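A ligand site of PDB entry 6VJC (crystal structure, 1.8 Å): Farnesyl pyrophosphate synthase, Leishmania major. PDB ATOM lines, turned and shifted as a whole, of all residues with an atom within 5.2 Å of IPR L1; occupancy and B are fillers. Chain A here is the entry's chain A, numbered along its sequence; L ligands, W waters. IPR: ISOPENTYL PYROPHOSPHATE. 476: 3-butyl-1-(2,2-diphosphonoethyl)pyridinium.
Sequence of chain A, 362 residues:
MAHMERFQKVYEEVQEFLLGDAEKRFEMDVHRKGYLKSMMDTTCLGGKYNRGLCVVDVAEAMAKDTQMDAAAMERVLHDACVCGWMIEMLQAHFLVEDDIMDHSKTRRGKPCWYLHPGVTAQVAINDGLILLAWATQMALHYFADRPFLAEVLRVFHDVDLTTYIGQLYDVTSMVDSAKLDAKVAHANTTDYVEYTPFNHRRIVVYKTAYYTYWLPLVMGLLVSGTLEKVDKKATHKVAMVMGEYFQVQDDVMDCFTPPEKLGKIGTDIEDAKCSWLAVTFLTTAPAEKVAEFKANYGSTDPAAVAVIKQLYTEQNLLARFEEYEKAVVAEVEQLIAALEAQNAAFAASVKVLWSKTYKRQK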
ATOM      1  N   GLY A  46      14.409  19.407  22.691  1.00  0.00           N
ATOM      2  CA  GLY A  46      14.718  19.027  24.082  1.00  0.00           C
ATOM      3  C   GLY A  46      15.475  17.728  24.209  1.00  0.00           C
ATOM      4  O   GLY A  46      15.881  17.435  25.330  1.00  0.00           O
ATOM      5  N   GLY A  47      15.623  16.942  23.146  1.00  0.00           N
ATOM      6  CA  GLY A  47      16.393  15.687  23.146  1.00  0.00           C
ATOM      7  C   GLY A  47      17.853  15.980  22.854  1.00  0.00           C
ATOM      8  O   GLY A  47      18.242  17.157  22.860  1.00  0.00           O
ATOM      9  N   LYS A  48      18.641  14.948  22.620  1.00  0.00           N
ATOM     10  CA  LYS A  48      20.108  15.115  22.470  1.00  0.00           C
ATOM     11  C   LYS A  48      20.450  15.400  21.001  1.00  0.00           C
ATOM     12  O   LYS A  48      21.578  15.860  20.736  1.00  0.00           O
ATOM     13  CB  LYS A  48      20.855  13.892  22.985  1.00  0.00           C
ATOM     14  CG  LYS A  48      20.559  13.462  24.421  1.00  0.00           C
ATOM     15  CD  LYS A  48      21.216  12.112  24.741  1.00  0.00           C
ATOM     16  CE  LYS A  48      20.379  10.875  24.374  1.00  0.00           C
ATOM     17  NZ  LYS A  48      19.154  10.801  25.209  1.00  0.00           N
ATOM     18  N   TYR A  49      19.529  15.141  20.072  1.00  0.00           N
ATOM     19  CA  TYR A  49      19.699  15.329  18.606  1.00  0.00           C
ATOM     20  C   TYR A  49      20.817  14.422  18.058  1.00  0.00           C
ATOM     21  O   TYR A  49      21.338  14.716  16.972  1.00  0.00           O
ATOM     22  CB  TYR A  49      19.901  16.806  18.226  1.00  0.00           C
ATOM     23  CG  TYR A  49      18.946  17.766  18.888  1.00  0.00           C
ATOM     24  CD1 TYR A  49      17.615  17.881  18.484  1.00  0.00           C
ATOM     25  CD2 TYR A  49      19.346  18.566  19.953  1.00  0.00           C
ATOM     26  CE1 TYR A  49      16.736  18.762  19.079  1.00  0.00           C
ATOM     27  CE2 TYR A  49      18.477  19.474  20.556  1.00  0.00           C
ATOM     28  CZ  TYR A  49      17.157  19.568  20.133  1.00  0.00           C
ATOM     29  OH  TYR A  49      16.310  20.478  20.771  1.00  0.00           O
ATOM     30  N   ARG A  51      20.519  11.555  16.557  1.00  0.00           N
ATOM     31  CA  ARG A  51      20.127  11.024  15.232  1.00  0.00           C
ATOM     32  C   ARG A  51      20.259  12.120  14.168  1.00  0.00           C
ATOM     33  O   ARG A  51      20.913  11.852  13.146  1.00  0.00           O
ATOM     34  CB  ARG A  51      18.702  10.466  15.271  1.00  0.00           C
ATOM     35  CG  ARG A  51      18.535   9.296  16.219  1.00  0.00           C
ATOM     36  CD  ARG A  51      17.057   8.985  16.374  1.00  0.00           C
ATOM     37  NE  ARG A  51      16.835   8.000  17.420  1.00  0.00           N
ATOM     38  CZ  ARG A  51      16.876   8.235  18.726  1.00  0.00           C
ATOM     39  NH1 ARG A  51      17.160   9.436  19.201  1.00  0.00           N
ATOM     40  NH2 ARG A  51      16.632   7.241  19.577  1.00  0.00           N
ATOM     41  N   GLU A  88      14.434  13.272  13.462  1.00  0.00           N
ATOM     42  CA  GLU A  88      13.992  13.876  14.751  1.00  0.00           C
ATOM     43  C   GLU A  88      12.464  13.898  14.814  1.00  0.00           C
ATOM     44  O   GLU A  88      11.954  13.689  15.901  1.00  0.00           O
ATOM     45  CB  GLU A  88      14.628  15.242  14.939  1.00  0.00           C
ATOM     46  CG  GLU A  88      16.129  15.136  15.186  1.00  0.00           C
ATOM     47  CD  GLU A  88      16.555  14.409  16.443  1.00  0.00           C
ATOM     48  OE1 GLU A  88      15.774  14.421  17.446  1.00  0.00           O
ATOM     49  OE2 GLU A  88      17.661  13.852  16.429  1.00  0.00           O
ATOM     50  N   GLN A  91      11.314  10.389  15.469  1.00  0.00           N
ATOM     51  CA  GLN A  91      11.546  10.184  16.913  1.00  0.00           C
ATOM     52  C   GLN A  91      10.394  10.832  17.684  1.00  0.00           C
ATOM     53  O   GLN A  91       9.830  10.163  18.546  1.00  0.00           O
ATOM     54  CB  GLN A  91      12.926  10.752  17.305  1.00  0.00           C
ATOM     55  CG  GLN A  91      13.138  10.901  18.800  1.00  0.00           C
ATOM     56  CD  GLN A  91      13.471   9.629  19.532  1.00  0.00           C
ATOM     57  OE1 GLN A  91      14.227   9.657  20.524  1.00  0.00           O
ATOM     58  NE2 GLN A  91      12.863   8.540  19.106  1.00  0.00           N
ATOM     59  N   LEU A  95       7.898   8.881  20.204  1.00  0.00           N
ATOM     60  CA  LEU A  95       7.853   9.127  21.670  1.00  0.00           C
ATOM     61  C   LEU A  95       6.439   9.569  22.044  1.00  0.00           C
ATOM     62  O   LEU A  95       5.970   9.178  23.116  1.00  0.00           O
ATOM     63  CB  LEU A  95       8.920  10.132  22.063  1.00  0.00           C
ATOM     64  CG  LEU A  95      10.368   9.734  21.723  1.00  0.00           C
ATOM     65  CD1 LEU A  95      11.320  10.675  22.448  1.00  0.00           C
ATOM     66  CD2 LEU A  95      10.661   8.303  22.147  1.00  0.00           C
ATOM     67  N   ARG A 107       8.707  13.362  29.802  1.00  0.00           N
ATOM     68  CA  ARG A 107       9.584  13.156  28.632  1.00  0.00           C
ATOM     69  C   ARG A 107      10.448  14.406  28.478  1.00  0.00           C
ATOM     70  O   ARG A 107       9.891  15.524  28.446  1.00  0.00           O
ATOM     71  CB  ARG A 107       8.755  12.895  27.364  1.00  0.00           C
ATOM     72  CG  ARG A 107       9.538  12.967  26.049  1.00  0.00           C
ATOM     73  CD  ARG A 107      10.463  11.750  25.932  1.00  0.00           C
ATOM     74  NE  ARG A 107       9.714  10.515  25.772  1.00  0.00           N
ATOM     75  CZ  ARG A 107      10.249   9.300  25.785  1.00  0.00           C
ATOM     76  NH1 ARG A 107      11.569   9.150  25.839  1.00  0.00           N
ATOM     77  NH2 ARG A 107       9.472   8.234  25.624  1.00  0.00           N
ATOM     78  N   ARG A 108      11.767  14.221  28.392  1.00  0.00           N
ATOM     79  CA  ARG A 108      12.767  15.316  28.187  1.00  0.00           C
ATOM     80  C   ARG A 108      12.537  16.396  29.252  1.00  0.00           C
ATOM     81  O   ARG A 108      12.539  17.571  28.922  1.00  0.00           O
ATOM     82  CB  ARG A 108      12.680  15.881  26.769  1.00  0.00           C
ATOM     83  CG  ARG A 108      13.157  14.894  25.720  1.00  0.00           C
ATOM     84  CD  ARG A 108      12.661  15.322  24.357  1.00  0.00           C
ATOM     85  NE  ARG A 108      13.143  14.439  23.295  1.00  0.00           N
ATOM     86  CZ  ARG A 108      12.743  14.527  22.025  1.00  0.00           C
ATOM     87  NH1 ARG A 108      11.867  15.466  21.692  1.00  0.00           N
ATOM     88  NH2 ARG A 108      13.208  13.696  21.107  1.00  0.00           N
ATOM     89  N   THR A 208      14.822  -0.180  18.111  1.00  0.00           N
ATOM     90  CA  THR A 208      15.787   0.923  18.366  1.00  0.00           C
ATOM     91  C   THR A 208      16.905   1.005  17.326  1.00  0.00           C
ATOM     92  O   THR A 208      17.178   2.120  16.887  1.00  0.00           O
ATOM     93  CB  THR A 208      16.411   0.813  19.767  1.00  0.00           C
ATOM     94  OG1 THR A 208      15.316   0.964  20.679  1.00  0.00           O
ATOM     95  CG2 THR A 208      17.510   1.858  19.988  1.00  0.00           C
ATOM     96  N   TYR A 211      16.289   2.719  13.500  1.00  0.00           N
ATOM     97  CA  TYR A 211      16.003   4.162  13.354  1.00  0.00           C
ATOM     98  C   TYR A 211      17.046   5.020  14.077  1.00  0.00           C
ATOM     99  O   TYR A 211      17.202   6.168  13.658  1.00  0.00           O
ATOM    100  CB  TYR A 211      14.586   4.494  13.832  1.00  0.00           C
ATOM    101  CG  TYR A 211      14.398   4.900  15.266  1.00  0.00           C
ATOM    102  CD1 TYR A 211      14.157   3.947  16.236  1.00  0.00           C
ATOM    103  CD2 TYR A 211      14.267   6.245  15.630  1.00  0.00           C
ATOM    104  CE1 TYR A 211      13.856   4.315  17.549  1.00  0.00           C
ATOM    105  CE2 TYR A 211      13.966   6.627  16.933  1.00  0.00           C
ATOM    106  CZ  TYR A 211      13.766   5.656  17.901  1.00  0.00           C
ATOM    107  OH  TYR A 211      13.442   6.007  19.189  1.00  0.00           O
ATOM    108  N   THR A 212      17.782   4.475  15.049  1.00  0.00           N
ATOM    109  CA  THR A 212      18.723   5.274  15.883  1.00  0.00           C
ATOM    110  C   THR A 212      20.140   5.259  15.293  1.00  0.00           C
ATOM    111  O   THR A 212      20.870   6.285  15.426  1.00  0.00           O
ATOM    112  CB  THR A 212      18.665   4.863  17.370  1.00  0.00           C
ATOM    113  OG1 THR A 212      17.308   4.898  17.812  1.00  0.00           O
ATOM    114  CG2 THR A 212      19.448   5.811  18.267  1.00  0.00           C
ATOM    115  N   PHE A 246      23.031   0.672  22.762  1.00  0.00           N
ATOM    116  CA  PHE A 246      22.301   1.918  23.102  1.00  0.00           C
ATOM    117  C   PHE A 246      21.030   1.565  23.879  1.00  0.00           C
ATOM    118  O   PHE A 246      20.723   2.230  24.893  1.00  0.00           O
ATOM    119  CB  PHE A 246      21.996   2.737  21.860  1.00  0.00           C
ATOM    120  CG  PHE A 246      21.200   3.994  22.142  1.00  0.00           C
ATOM    121  CD1 PHE A 246      21.852   5.194  22.406  1.00  0.00           C
ATOM    122  CD2 PHE A 246      19.819   3.971  22.110  1.00  0.00           C
ATOM    123  CE1 PHE A 246      21.131   6.344  22.640  1.00  0.00           C
ATOM    124  CE2 PHE A 246      19.100   5.124  22.369  1.00  0.00           C
ATOM    125  CZ  PHE A 246      19.751   6.313  22.597  1.00  0.00           C
ATOM    126  N   GLN A 247      20.247   0.596  23.414  1.00  0.00           N
ATOM    127  CA  GLN A 247      18.970   0.247  24.109  1.00  0.00           C
ATOM    128  C   GLN A 247      19.253  -0.505  25.423  1.00  0.00           C
ATOM    129  O   GLN A 247      18.515  -0.350  26.381  1.00  0.00           O
ATOM    130  CB  GLN A 247      18.053  -0.593  23.228  1.00  0.00           C
ATOM    131  CG  GLN A 247      16.691  -0.812  23.840  1.00  0.00           C
ATOM    132  CD  GLN A 247      16.009   0.497  24.131  1.00  0.00           C
ATOM    133  OE1 GLN A 247      15.948   1.351  23.275  1.00  0.00           O
ATOM    134  NE2 GLN A 247      15.481   0.643  25.338  1.00  0.00           N
ATOM    135  N   ASP A 250      19.800   2.217  27.823  1.00  0.00           N
ATOM    136  CA  ASP A 250      18.472   2.790  28.128  1.00  0.00           C
ATOM    137  C   ASP A 250      17.773   1.895  29.174  1.00  0.00           C
ATOM    138  O   ASP A 250      17.191   2.417  30.119  1.00  0.00           O
ATOM    139  CB  ASP A 250      17.679   2.948  26.845  1.00  0.00           C
ATOM    140  CG  ASP A 250      16.388   3.678  27.103  1.00  0.00           C
ATOM    141  OD1 ASP A 250      16.477   4.901  27.337  1.00  0.00           O
ATOM    142  OD2 ASP A 250      15.339   2.998  27.131  1.00  0.00           O
ATOM    143  N   LYS A 264      12.972  11.439  32.192  1.00  0.00           N
ATOM    144  CA  LYS A 264      11.776  10.577  32.024  1.00  0.00           C
ATOM    145  C   LYS A 264      11.721   9.610  33.185  1.00  0.00           C
ATOM    146  O   LYS A 264      12.782   9.353  33.763  1.00  0.00           O
ATOM    147  CB  LYS A 264      11.825   9.797  30.713  1.00  0.00           C
ATOM    148  CG  LYS A 264      13.027   8.896  30.508  1.00  0.00           C
ATOM    149  CD  LYS A 264      13.182   8.371  29.104  1.00  0.00           C
ATOM    150  CE  LYS A 264      14.318   7.365  29.037  1.00  0.00           C
ATOM    151  NZ  LYS A 264      14.642   6.990  27.644  1.00  0.00           N
ATOM    152  N   ARG A 360      27.613   7.039  27.699  1.00  0.00           N
ATOM    153  CA  ARG A 360      26.670   8.147  27.901  1.00  0.00           C
ATOM    154  C   ARG A 360      26.004   7.966  29.259  1.00  0.00           C
ATOM    155  O   ARG A 360      25.892   6.802  29.747  1.00  0.00           O
ATOM    156  CB  ARG A 360      25.654   8.233  26.754  1.00  0.00           C
ATOM    157  CG  ARG A 360      24.621   7.121  26.803  1.00  0.00           C
ATOM    158  CD  ARG A 360      23.887   7.085  25.479  1.00  0.00           C
ATOM    159  NE  ARG A 360      22.877   6.014  25.476  1.00  0.00           N
ATOM    160  CZ  ARG A 360      21.590   6.151  25.747  1.00  0.00           C
ATOM    161  NH1 ARG A 360      21.077   7.324  26.096  1.00  0.00           N
ATOM    162  NH2 ARG A 360      20.799   5.088  25.669  1.00  0.00           N
ATOM    163  N   LYS A 362      22.880   9.815  29.853  1.00  0.00           N
ATOM    164  CA  LYS A 362      21.442  10.111  29.599  1.00  0.00           C
ATOM    165  C   LYS A 362      21.152   9.996  28.099  1.00  0.00           C
ATOM    166  O   LYS A 362      19.964  10.146  27.752  1.00  0.00           O
ATOM    167  CB  LYS A 362      21.039  11.484  30.137  1.00  0.00           C
ATOM    168  CG  LYS A 362      21.748  12.698  29.543  1.00  0.00           C
ATOM    169  CD  LYS A 362      20.973  14.023  29.762  1.00  0.00           C
ATOM    170  CE  LYS A 362      19.853  14.206  28.736  1.00  0.00           C
ATOM    171  NZ  LYS A 362      19.084  15.457  28.930  1.00  0.00           N
ATOM    172  OXT LYS A 362      22.104   9.744  27.307  1.00  0.00           O
HETATM  173  P11 IPR L   1      16.120  11.969  22.904  1.00  0.00           P
HETATM  174  O14 IPR L   1      15.275  12.604  23.954  1.00  0.00           O
HETATM  175  O12 IPR L   1      17.664  12.270  22.908  1.00  0.00           O
HETATM  176  O13 IPR L   1      15.593  12.084  21.464  1.00  0.00           O
HETATM  177  O10 IPR L   1      15.902  10.386  23.244  1.00  0.00           O
HETATM  178  P7  IPR L   1      16.844   9.077  23.037  1.00  0.00           P
HETATM  179  O8  IPR L   1      17.539   8.691  24.353  1.00  0.00           O
HETATM  180  O9  IPR L   1      17.783   9.251  21.907  1.00  0.00           O
HETATM  181  O6  IPR L   1      15.775   7.990  22.579  1.00  0.00           O
HETATM  182  C5  IPR L   1      14.697   7.605  23.413  1.00  0.00           C
HETATM  183  C4  IPR L   1      14.110   6.323  22.847  1.00  0.00           C
HETATM  184  C2  IPR L   1      15.047   5.098  22.850  1.00  0.00           C
HETATM  185  C1  IPR L   1      15.410   4.540  21.521  1.00  0.00           C
HETATM  186  C3  IPR L   1      15.812   4.758  24.104  1.00  0.00           C
HETATM  187  O11 476 L   2      12.440   6.495  25.877  1.00  0.00           O
HETATM  188  P10 476 L   2      11.679   5.322  26.446  1.00  0.00           P
HETATM  189  O13 476 L   2      10.230   5.691  26.704  1.00  0.00           O
HETATM  190  O12 476 L   2      12.294   4.776  27.660  1.00  0.00           O
HETATM  191  C8  476 L   2      11.757   3.989  25.165  1.00  0.00           C
HETATM  192  P9  476 L   2      11.090   2.389  25.705  1.00  0.00           P
HETATM  193  O15 476 L   2       9.664   2.550  26.130  1.00  0.00           O
HETATM  194  O14 476 L   2      11.165   1.427  24.509  1.00  0.00           O
HETATM  195  O16 476 L   2      11.937   1.899  26.822  1.00  0.00           O
HETATM  196  C7  476 L   2      11.022   4.581  23.969  1.00  0.00           C
HETATM  197  N2  476 L   2      11.174   3.873  22.685  1.00  0.00           N
HETATM  198  C1  476 L   2      10.101   3.863  21.818  1.00  0.00           C
HETATM  199  C6  476 L   2      10.205   3.341  20.546  1.00  0.00           C
HETATM  200  C5  476 L   2      11.356   2.630  20.236  1.00  0.00           C
HETATM  201  C4  476 L   2      12.416   2.622  21.106  1.00  0.00           C
HETATM  202  C3  476 L   2      12.313   3.267  22.343  1.00  0.00           C
HETATM  203  C17 476 L   2       9.142   3.616  19.512  1.00  0.00           C
HETATM  204  C18 476 L   2       7.993   2.653  19.385  1.00  0.00           C
HETATM  205  C19 476 L   2       6.968   3.025  18.312  1.00  0.00           C
HETATM  206  C20 476 L   2       5.725   3.667  18.828  1.00  0.00           C
HETATM  207  O   HOH W   1      20.253   9.229  20.986  1.00  0.00           O
HETATM  208  O   HOH W   2      19.181  11.851  20.632  1.00  0.00           O
HETATM  209  O   HOH W   3      17.056  13.053  26.083  1.00  0.00           O
HETATM  210  O   HOH W   4      16.577  14.163  19.959  1.00  0.00           O
HETATM  211  O   HOH W   5      15.909   9.322  26.574  1.00  0.00           O
HETATM  212  O   HOH W   6      18.227   6.575  26.123  1.00  0.00           O
HETATM  213  O   HOH W   7      13.892  11.034  25.716  1.00  0.00           O
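Water W7 lies within hydrogen-bond range of an oxygen (O14) of IPR L1 (2.7 Å) and the guanidinium group (NH1) of Arg 107 (3.0 Å). Water W4 lies within hydrogen-bond range of the side-chain carboxylate (OE1) of Glu 88, an oxygen (O13) of IPR L1, the backbone NH (N) of Tyr 49 and the backbone NH (N) of Lys 48. Water W2 lies within hydrogen-bond range of an oxygen (O12) of IPR L1 (2.8 Å), the backbone NH of Tyr 49 (3.4 Å) and the guanidinium group of Arg 51 (3.5 Å). Water W3 lies within hydrogen-bond range of an oxygen (O14) of IPR L1 (2.8 Å) and the side-chain amino group (NZ) of Lys 48 (3.2 Å). Water W5 lies within hydrogen-bond range of O8 of IPR L1 and NZ of Lys 264. Water W6 lies within hydrogen-bond range of OD1 of Asp 250 (2.7 Å), O8 of IPR L1 (2.8 Å) and NH1 of Arg 360 (2.9 Å).
The side-chain amide oxygen (OE1) of Gln 91 lies close to an oxygen (O13) of IPR L1. An oxygen (O11) of 476 L2 is in salt-bridge range of the side-chain amino group (NZ) of Lys 264 (2.9 Å). The guanidinium group (NH1) of Arg 51 lies within salt-bridge range of an oxygen (O9) of IPR L1, 2.8 Å away. The backbone NH of Lys 48 is in hydrogen-bond range of an oxygen (O12) of IPR L1 (2.9 Å). The guanidinium group of Arg 108 lies within salt-bridge range of an oxygen (O14) of IPR L1, at 2.9 Å. NZ of Lys 48 lies within salt-bridge range of O8 of IPR L1 (2.8 Å). NH1 of Arg 107 lies within salt-bridge range of O11 of 476 L2 (2.8 Å).
Gly 47 touches IPR L1 (CA to O14, 3.4 Å). Thr 208 touches IPR L1. OH of Tyr 211 touches C1 of IPR L1, 3.4 Å away. Phe 246 touches IPR L1 (CZ to O9, 3.6 Å). OE1 of Gln 247 touches C3 of IPR L1 (3.5 Å). CG of Asp 250 touches C3 of IPR L1, 3.2 Å away. Hydrophobic or aromatic side chains that line IPR L1: Phe 246. Of the 19 residues printed, 10 come within 4 Å of IPR L1. The nearest printed residue that does not touch IPR L1 is Leu 95 (4.04 Å).
The side-chain hydroxyl of Thr 208 lies within hydrogen-bond range of the side-chain amide oxygen of Gln 247 (2.7 Å). The side-chain amino group of Lys 48 is in salt-bridge range of the chain-end carboxylate of Lys 362, at 2.7 Å. The guanidinium group (NH1) of Arg 51 sits at hydrogen-bond distance from the side-chain amide oxygen (OE1) of Gln 91, 3.2 Å away. The side-chain amino group of Lys 264 is in salt-bridge range of the side-chain carboxylate of Asp 250 (2.8 Å). The side-chain hydroxyl of Tyr 211 lies within hydrogen-bond range of the guanidinium group of Arg 51 (3.4 Å). The side-chain carboxylate (OD2) of Asp 250 sits close to the side-chain amide nitrogen (NE2) of Gln 247, 3.0 Å away. OG1 of Thr 212 is in hydrogen-bond range of O of Thr 208, at 2.9 Å. The side-chain amide nitrogen (NE2) of Gln 91 lies within hydrogen-bond range of the side-chain hydroxyl (OH) of Tyr 211.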
